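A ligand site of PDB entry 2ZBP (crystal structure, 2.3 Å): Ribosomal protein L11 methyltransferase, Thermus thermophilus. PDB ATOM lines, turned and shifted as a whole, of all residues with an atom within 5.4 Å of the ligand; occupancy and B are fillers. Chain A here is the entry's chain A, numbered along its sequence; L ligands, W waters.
The backbone carbonyl oxygen (O) of Thr 129 is in hydrogen-bond range of a nitrogen (N1) of the ligand, 3.4 Å away.
An oxygen (O5) of the ligand sits at hydrogen-bond distance from the side-chain carboxylate (OD2) of Asp 149 (2.5 Å).
The side-chain amide nitrogen (ND2) of Asn 191 is in hydrogen-bond range of an oxygen (O1) of the ligand.
O2 of the ligand lies within hydrogen-bond range of OG1 of Thr 107 (2.4 Å).
O of Gly 128 lies within hydrogen-bond range of N1 of the ligand.
N5 of the ligand is in hydrogen-bond range of OG of Ser 175 (3.1 Å).
N of Ile 150 lies within hydrogen-bond range of O of Gly 174 (3.3 Å).
The backbone NH of Ser 131 sits at hydrogen-bond distance from the backbone carbonyl oxygen of Phe 99, at 2.8 Å.
OG1 of Thr 129 lies within hydrogen-bond range of OD2 of Asp 126, at 3.1 Å.
The side-chain carboxylate (OD2) of Asp 149 sits at hydrogen-bond distance from the backbone NH (N) of Asp 151 (2.8 Å).
The side-chain amide nitrogen (ND2) of Asn 191 lies within hydrogen-bond range of the side-chain hydroxyl (OG1) of Thr 106 (2.6 Å).
The backbone carbonyl oxygen of Val 148 sits at hydrogen-bond distance from the backbone NH of Thr 129 (2.9 Å).
O of Asp 149 sits at hydrogen-bond distance from N of Gly 174, 2.8 Å away.
The backbone carbonyl oxygen (O) of Gly 100 sits at hydrogen-bond distance from the side-chain hydroxyl (OG) of Ser 131, at 2.9 Å.
Phe 99 touches the ligand.
Gly 100 touches the ligand.
CD2 of Leu 127 touches C14 of the ligand (3.6 Å).
Gly 130 touches the ligand.
Leu 134 touches the ligand.
Ile 150 touches the ligand (N to N6, 3.7 Å).
Asp 151 touches the ligand.
Gly 174 touches the ligand.
CD2 of Leu 192 touches O3 of the ligand, at 3.7 Å.
CD2 of Leu 196 touches N4 of the ligand (3.6 Å).
Hydrophobic or aromatic side chains within 4 Å of the ligand: Phe 99, Leu 127, Leu 134, Ile 150, Leu 192 and Leu 196.
Of the 25 residues printed, 16 come within 4 Å of the ligand.
The nearest printed residue that does not touch the ligand is Val 133 (4.1 Å).
Water W6 bridges an oxygen (O5) of the ligand (2.7 Å) and the side-chain carboxylate of Asp 151 (2.9 Å).
Water W7 lies within hydrogen-bond range of O of Thr 129, OD2 of Asp 126, N1 of the ligand, N of Leu 134 and N of Val 133.
Water W4 bridges OG of Ser 175 and N4 of the ligand.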
ATOM      1  N   PHE A  99      20.804 -32.403  -1.140  1.00  0.00           N
ATOM      2  CA  PHE A  99      22.242 -32.303  -0.884  1.00  0.00           C
ATOM      3  C   PHE A  99      22.575 -31.089  -0.014  1.00  0.00           C
ATOM      4  O   PHE A  99      22.060 -29.990  -0.230  1.00  0.00           O
ATOM      5  CB  PHE A  99      23.013 -32.224  -2.214  1.00  0.00           C
ATOM      6  CG  PHE A  99      24.488 -32.562  -2.109  1.00  0.00           C
ATOM      7  CD1 PHE A  99      25.317 -31.897  -1.210  1.00  0.00           C
ATOM      8  CD2 PHE A  99      25.050 -33.518  -2.940  1.00  0.00           C
ATOM      9  CE1 PHE A  99      26.681 -32.174  -1.138  1.00  0.00           C
ATOM     10  CE2 PHE A  99      26.419 -33.808  -2.868  1.00  0.00           C
ATOM     11  CZ  PHE A  99      27.234 -33.133  -1.970  1.00  0.00           C
ATOM     12  N   GLY A 100      23.432 -31.317   0.975  1.00  0.00           N
ATOM     13  CA  GLY A 100      23.830 -30.252   1.873  1.00  0.00           C
ATOM     14  C   GLY A 100      23.828 -30.703   3.316  1.00  0.00           C
ATOM     15  O   GLY A 100      23.544 -29.917   4.224  1.00  0.00           O
ATOM     16  N   THR A 101      24.125 -31.982   3.532  1.00  0.00           N
ATOM     17  CA  THR A 101      24.164 -32.533   4.886  1.00  0.00           C
ATOM     18  C   THR A 101      25.413 -32.084   5.628  1.00  0.00           C
ATOM     19  O   THR A 101      25.438 -32.081   6.853  1.00  0.00           O
ATOM     20  CB  THR A 101      24.137 -34.077   4.850  1.00  0.00           C
ATOM     21  OG1 THR A 101      25.320 -34.552   4.194  1.00  0.00           O
ATOM     22  CG2 THR A 101      22.903 -34.567   4.095  1.00  0.00           C
ATOM     23  N   THR A 106      32.927 -31.079  -0.595  1.00  0.00           N
ATOM     24  CA  THR A 106      32.637 -29.812  -1.265  1.00  0.00           C
ATOM     25  C   THR A 106      31.880 -28.826  -0.368  1.00  0.00           C
ATOM     26  O   THR A 106      32.218 -27.638  -0.322  1.00  0.00           O
ATOM     27  CB  THR A 106      31.848 -30.040  -2.566  1.00  0.00           C
ATOM     28  OG1 THR A 106      30.629 -30.737  -2.288  1.00  0.00           O
ATOM     29  CG2 THR A 106      32.679 -30.866  -3.548  1.00  0.00           C
ATOM     30  N   THR A 107      30.881 -29.322   0.343  1.00  0.00           N
ATOM     31  CA  THR A 107      30.101 -28.498   1.245  1.00  0.00           C
ATOM     32  C   THR A 107      31.009 -27.900   2.287  1.00  0.00           C
ATOM     33  O   THR A 107      30.899 -26.716   2.622  1.00  0.00           O
ATOM     34  CB  THR A 107      29.073 -29.343   1.968  1.00  0.00           C
ATOM     35  OG1 THR A 107      28.327 -30.081   0.999  1.00  0.00           O
ATOM     36  CG2 THR A 107      28.151 -28.484   2.806  1.00  0.00           C
ATOM     37  N   ALA A 110      33.201 -25.175   0.853  1.00  0.00           N
ATOM     38  CA  ALA A 110      32.336 -24.012   0.680  1.00  0.00           C
ATOM     39  C   ALA A 110      32.147 -23.251   1.975  1.00  0.00           C
ATOM     40  O   ALA A 110      32.264 -22.028   2.014  1.00  0.00           O
ATOM     41  CB  ALA A 110      30.988 -24.435   0.120  1.00  0.00           C
ATOM     42  N   ASP A 126      23.394 -18.246  -3.458  1.00  0.00           N
ATOM     43  CA  ASP A 126      23.781 -19.645  -3.247  1.00  0.00           C
ATOM     44  C   ASP A 126      23.170 -20.414  -4.409  1.00  0.00           C
ATOM     45  O   ASP A 126      22.018 -20.815  -4.367  1.00  0.00           O
ATOM     46  CB  ASP A 126      23.220 -20.124  -1.903  1.00  0.00           C
ATOM     47  CG  ASP A 126      23.556 -21.588  -1.605  1.00  0.00           C
ATOM     48  OD1 ASP A 126      24.133 -22.281  -2.470  1.00  0.00           O
ATOM     49  OD2 ASP A 126      23.218 -22.042  -0.472  1.00  0.00           O
ATOM     50  N   LEU A 127      23.951 -20.590  -5.468  1.00  0.00           N
ATOM     51  CA  LEU A 127      23.506 -21.271  -6.676  1.00  0.00           C
ATOM     52  C   LEU A 127      23.469 -22.781  -6.501  1.00  0.00           C
ATOM     53  O   LEU A 127      24.518 -23.423  -6.445  1.00  0.00           O
ATOM     54  CB  LEU A 127      24.455 -20.946  -7.826  1.00  0.00           C
ATOM     55  CG  LEU A 127      23.887 -20.582  -9.198  1.00  0.00           C
ATOM     56  CD1 LEU A 127      24.915 -20.970 -10.253  1.00  0.00           C
ATOM     57  CD2 LEU A 127      22.562 -21.277  -9.450  1.00  0.00           C
ATOM     58  N   GLY A 128      22.261 -23.341  -6.457  1.00  0.00           N
ATOM     59  CA  GLY A 128      22.105 -24.777  -6.272  1.00  0.00           C
ATOM     60  C   GLY A 128      22.162 -24.999  -4.766  1.00  0.00           C
ATOM     61  O   GLY A 128      22.933 -25.802  -4.255  1.00  0.00           O
ATOM     62  N   THR A 129      21.328 -24.236  -4.076  1.00  0.00           N
ATOM     63  CA  THR A 129      21.239 -24.247  -2.621  1.00  0.00           C
ATOM     64  C   THR A 129      20.950 -25.605  -1.980  1.00  0.00           C
ATOM     65  O   THR A 129      21.308 -25.835  -0.828  1.00  0.00           O
ATOM     66  CB  THR A 129      20.189 -23.195  -2.158  1.00  0.00           C
ATOM     67  OG1 THR A 129      20.308 -22.980  -0.754  1.00  0.00           O
ATOM     68  CG2 THR A 129      18.767 -23.657  -2.505  1.00  0.00           C
ATOM     69  N   GLY A 130      20.341 -26.515  -2.722  1.00  0.00           N
ATOM     70  CA  GLY A 130      20.019 -27.812  -2.155  1.00  0.00           C
ATOM     71  C   GLY A 130      19.329 -27.687  -0.803  1.00  0.00           C
ATOM     72  O   GLY A 130      18.217 -27.163  -0.694  1.00  0.00           O
ATOM     73  N   SER A 131      20.019 -28.165   0.233  1.00  0.00           N
ATOM     74  CA  SER A 131      19.498 -28.143   1.595  1.00  0.00           C
ATOM     75  C   SER A 131      19.469 -26.725   2.173  1.00  0.00           C
ATOM     76  O   SER A 131      18.817 -26.487   3.209  1.00  0.00           O
ATOM     77  CB  SER A 131      20.369 -29.020   2.500  1.00  0.00           C
ATOM     78  OG  SER A 131      21.549 -28.344   2.887  1.00  0.00           O
ATOM     79  N   VAL A 133      22.142 -25.124   3.269  1.00  0.00           N
ATOM     80  CA  VAL A 133      23.200 -24.955   4.269  1.00  0.00           C
ATOM     81  C   VAL A 133      24.128 -23.771   4.005  1.00  0.00           C
ATOM     82  O   VAL A 133      24.444 -23.021   4.917  1.00  0.00           O
ATOM     83  CB  VAL A 133      24.079 -26.255   4.408  1.00  0.00           C
ATOM     84  CG1 VAL A 133      24.678 -26.660   3.061  1.00  0.00           C
ATOM     85  CG2 VAL A 133      25.205 -25.998   5.408  1.00  0.00           C
ATOM     86  N   LEU A 134      24.569 -23.577   2.763  1.00  0.00           N
ATOM     87  CA  LEU A 134      25.469 -22.439   2.503  1.00  0.00           C
ATOM     88  C   LEU A 134      24.730 -21.098   2.733  1.00  0.00           C
ATOM     89  O   LEU A 134      25.261 -20.185   3.396  1.00  0.00           O
ATOM     90  CB  LEU A 134      26.051 -22.533   1.076  1.00  0.00           C
ATOM     91  CG  LEU A 134      26.839 -23.832   0.751  1.00  0.00           C
ATOM     92  CD1 LEU A 134      27.462 -23.734  -0.630  1.00  0.00           C
ATOM     93  CD2 LEU A 134      27.933 -24.088   1.791  1.00  0.00           C
ATOM     94  N   VAL A 148      18.958 -20.523  -4.594  1.00  0.00           N
ATOM     95  CA  VAL A 148      18.101 -20.966  -5.695  1.00  0.00           C
ATOM     96  C   VAL A 148      18.470 -22.369  -6.132  1.00  0.00           C
ATOM     97  O   VAL A 148      19.595 -22.828  -5.934  1.00  0.00           O
ATOM     98  CB  VAL A 148      18.194 -20.013  -6.895  1.00  0.00           C
ATOM     99  CG1 VAL A 148      18.007 -18.566  -6.411  1.00  0.00           C
ATOM    100  CG2 VAL A 148      19.528 -20.183  -7.600  1.00  0.00           C
ATOM    101  N   ASP A 149      17.528 -23.061  -6.758  1.00  0.00           N
ATOM    102  CA  ASP A 149      17.769 -24.423  -7.202  1.00  0.00           C
ATOM    103  C   ASP A 149      16.736 -24.756  -8.263  1.00  0.00           C
ATOM    104  O   ASP A 149      15.584 -24.378  -8.144  1.00  0.00           O
ATOM    105  CB  ASP A 149      17.591 -25.373  -6.010  1.00  0.00           C
ATOM    106  CG  ASP A 149      18.279 -26.692  -6.210  1.00  0.00           C
ATOM    107  OD1 ASP A 149      19.186 -27.014  -5.416  1.00  0.00           O
ATOM    108  OD2 ASP A 149      17.926 -27.411  -7.168  1.00  0.00           O
ATOM    109  N   ILE A 150      17.160 -25.473  -9.300  1.00  0.00           N
ATOM    110  CA  ILE A 150      16.209 -25.839 -10.340  1.00  0.00           C
ATOM    111  C   ILE A 150      15.312 -26.985  -9.866  1.00  0.00           C
ATOM    112  O   ILE A 150      14.347 -27.352 -10.545  1.00  0.00           O
ATOM    113  CB  ILE A 150      16.914 -26.299 -11.633  1.00  0.00           C
ATOM    114  CG1 ILE A 150      17.923 -27.397 -11.318  1.00  0.00           C
ATOM    115  CG2 ILE A 150      17.562 -25.103 -12.302  1.00  0.00           C
ATOM    116  CD1 ILE A 150      18.504 -28.056 -12.539  1.00  0.00           C
ATOM    117  N   ASP A 151      15.623 -27.540  -8.705  1.00  0.00           N
ATOM    118  CA  ASP A 151      14.830 -28.636  -8.164  1.00  0.00           C
ATOM    119  C   ASP A 151      13.904 -28.118  -7.049  1.00  0.00           C
ATOM    120  O   ASP A 151      14.347 -27.840  -5.925  1.00  0.00           O
ATOM    121  CB  ASP A 151      15.748 -29.742  -7.645  1.00  0.00           C
ATOM    122  CG  ASP A 151      14.972 -30.952  -7.131  1.00  0.00           C
ATOM    123  OD1 ASP A 151      13.753 -31.044  -7.395  1.00  0.00           O
ATOM    124  OD2 ASP A 151      15.589 -31.813  -6.479  1.00  0.00           O
ATOM    125  N   VAL A 154      13.594 -29.481  -3.113  1.00  0.00           N
ATOM    126  CA  VAL A 154      14.515 -29.130  -2.041  1.00  0.00           C
ATOM    127  C   VAL A 154      14.150 -27.891  -1.233  1.00  0.00           C
ATOM    128  O   VAL A 154      14.486 -27.793  -0.049  1.00  0.00           O
ATOM    129  CB  VAL A 154      15.986 -28.955  -2.563  1.00  0.00           C
ATOM    130  CG1 VAL A 154      16.398 -30.172  -3.387  1.00  0.00           C
ATOM    131  CG2 VAL A 154      16.141 -27.651  -3.380  1.00  0.00           C
ATOM    132  N   GLY A 174      14.761 -22.126  -9.643  1.00  0.00           N
ATOM    133  CA  GLY A 174      15.417 -21.537 -10.794  1.00  0.00           C
ATOM    134  C   GLY A 174      16.926 -21.598 -10.743  1.00  0.00           C
ATOM    135  O   GLY A 174      17.512 -22.232  -9.859  1.00  0.00           O
ATOM    136  N   SER A 175      17.561 -20.935 -11.710  1.00  0.00           N
ATOM    137  CA  SER A 175      19.011 -20.901 -11.779  1.00  0.00           C
ATOM    138  C   SER A 175      19.539 -19.473 -11.657  1.00  0.00           C
ATOM    139  O   SER A 175      18.938 -18.646 -10.979  1.00  0.00           O
ATOM    140  CB  SER A 175      19.503 -21.517 -13.094  1.00  0.00           C
ATOM    141  OG  SER A 175      20.919 -21.588 -13.130  1.00  0.00           O
ATOM    142  N   LEU A 176      20.660 -19.212 -12.321  1.00  0.00           N
ATOM    143  CA  LEU A 176      21.311 -17.905 -12.307  1.00  0.00           C
ATOM    144  C   LEU A 176      20.412 -16.771 -12.789  1.00  0.00           C
ATOM    145  O   LEU A 176      20.415 -15.691 -12.200  1.00  0.00           O
ATOM    146  CB  LEU A 176      22.576 -17.976 -13.154  1.00  0.00           C
ATOM    147  CG  LEU A 176      23.679 -16.936 -12.925  1.00  0.00           C
ATOM    148  CD1 LEU A 176      24.083 -16.904 -11.471  1.00  0.00           C
ATOM    149  CD2 LEU A 176      24.861 -17.307 -13.788  1.00  0.00           C
ATOM    150  N   ASN A 191      28.159 -24.825  -5.583  1.00  0.00           N
ATOM    151  CA  ASN A 191      28.678 -26.195  -5.509  1.00  0.00           C
ATOM    152  C   ASN A 191      27.965 -26.964  -6.609  1.00  0.00           C
ATOM    153  O   ASN A 191      26.839 -27.464  -6.415  1.00  0.00           O
ATOM    154  CB  ASN A 191      28.348 -26.817  -4.148  1.00  0.00           C
ATOM    155  CG  ASN A 191      29.025 -28.163  -3.944  1.00  0.00           C
ATOM    156  OD1 ASN A 191      29.379 -28.847  -4.910  1.00  0.00           O
ATOM    157  ND2 ASN A 191      29.185 -28.562  -2.691  1.00  0.00           N
ATOM    158  N   LEU A 192      28.611 -27.045  -7.774  1.00  0.00           N
ATOM    159  CA  LEU A 192      28.051 -27.745  -8.923  1.00  0.00           C
ATOM    160  C   LEU A 192      29.118 -28.697  -9.448  1.00  0.00           C
ATOM    161  O   LEU A 192      29.446 -29.685  -8.775  1.00  0.00           O
ATOM    162  CB  LEU A 192      27.635 -26.724  -9.989  1.00  0.00           C
ATOM    163  CG  LEU A 192      26.703 -25.634  -9.458  1.00  0.00           C
ATOM    164  CD1 LEU A 192      26.544 -24.478 -10.463  1.00  0.00           C
ATOM    165  CD2 LEU A 192      25.350 -26.259  -9.130  1.00  0.00           C
ATOM    166  N   LEU A 196      29.993 -27.199 -15.794  1.00  0.00           N
ATOM    167  CA  LEU A 196      28.932 -26.194 -15.716  1.00  0.00           C
ATOM    168  C   LEU A 196      29.474 -24.833 -15.301  1.00  0.00           C
ATOM    169  O   LEU A 196      29.052 -23.796 -15.828  1.00  0.00           O
ATOM    170  CB  LEU A 196      27.817 -26.636 -14.753  1.00  0.00           C
ATOM    171  CG  LEU A 196      26.585 -25.724 -14.565  1.00  0.00           C
ATOM    172  CD1 LEU A 196      25.995 -25.329 -15.917  1.00  0.00           C
ATOM    173  CD2 LEU A 196      25.533 -26.431 -13.709  1.00  0.00           C
HETATM  174  N1  LIG L   1      24.565 -26.341  -1.804  1.00  0.00           N
HETATM  175  C1  LIG L   1      24.841 -27.640  -1.107  1.00  0.00           C
HETATM  176  C2  LIG L   1      26.256 -27.687  -0.568  1.00  0.00           C
HETATM  177  O1  LIG L   1      27.012 -26.723  -0.742  1.00  0.00           O
HETATM  178  O2  LIG L   1      26.546 -28.769   0.038  1.00  0.00           O
HETATM  179  C3  LIG L   1      24.712 -28.838  -2.056  1.00  0.00           C
HETATM  180  C4  LIG L   1      24.441 -28.471  -3.455  1.00  0.00           C
HETATM  181  S1  LIG L   1      24.323 -29.821  -4.673  1.00  0.00           S
HETATM  182  C5  LIG L   1      26.051 -30.334  -4.863  1.00  0.00           C
HETATM  183  C6  LIG L   1      23.958 -28.944  -6.117  1.00  0.00           C
HETATM  184  C7  LIG L   1      22.519 -28.461  -6.190  1.00  0.00           C
HETATM  185  O3  LIG L   1      22.439 -27.695  -7.393  1.00  0.00           O
HETATM  186  C8  LIG L   1      21.533 -29.619  -6.387  1.00  0.00           C
HETATM  187  O4  LIG L   1      20.678 -29.580  -5.207  1.00  0.00           O
HETATM  188  C9  LIG L   1      20.716 -29.306  -7.634  1.00  0.00           C
HETATM  189  O5  LIG L   1      19.315 -29.468  -7.638  1.00  0.00           O
HETATM  190  C10 LIG L   1      21.233 -27.906  -8.046  1.00  0.00           C
HETATM  191  N2  LIG L   1      21.545 -27.690  -9.436  1.00  0.00           N
HETATM  192  C11 LIG L   1      22.054 -28.534 -10.401  1.00  0.00           C
HETATM  193  N3  LIG L   1      22.220 -27.957 -11.565  1.00  0.00           N
HETATM  194  C12 LIG L   1      21.787 -26.647 -11.354  1.00  0.00           C
HETATM  195  C13 LIG L   1      21.700 -25.501 -12.202  1.00  0.00           C
HETATM  196  N4  LIG L   1      22.077 -25.522 -13.493  1.00  0.00           N
HETATM  197  N5  LIG L   1      21.210 -24.311 -11.677  1.00  0.00           N
HETATM  198  C14 LIG L   1      20.832 -24.290 -10.371  1.00  0.00           C
HETATM  199  N6  LIG L   1      20.875 -25.308  -9.492  1.00  0.00           N
HETATM  200  C15 LIG L   1      21.359 -26.471 -10.046  1.00  0.00           C
HETATM  201  O   HOH W   1      23.011 -30.149 -13.657  1.00  0.00           O
HETATM  202  O   HOH W   2      25.865 -24.062  -3.880  1.00  0.00           O
HETATM  203  O   HOH W   3      21.948 -28.192 -14.874  1.00  0.00           O
HETATM  204  O   HOH W   4      21.585 -22.818 -15.408  1.00  0.00           O
HETATM  205  O   HOH W   5      29.181 -31.303  -5.637  1.00  0.00           O
HETATM  206  O   HOH W   6      18.425 -31.839  -6.857  1.00  0.00           O
HETATM  207  O   HOH W   7      23.373 -24.658   0.101  1.00  0.00           O
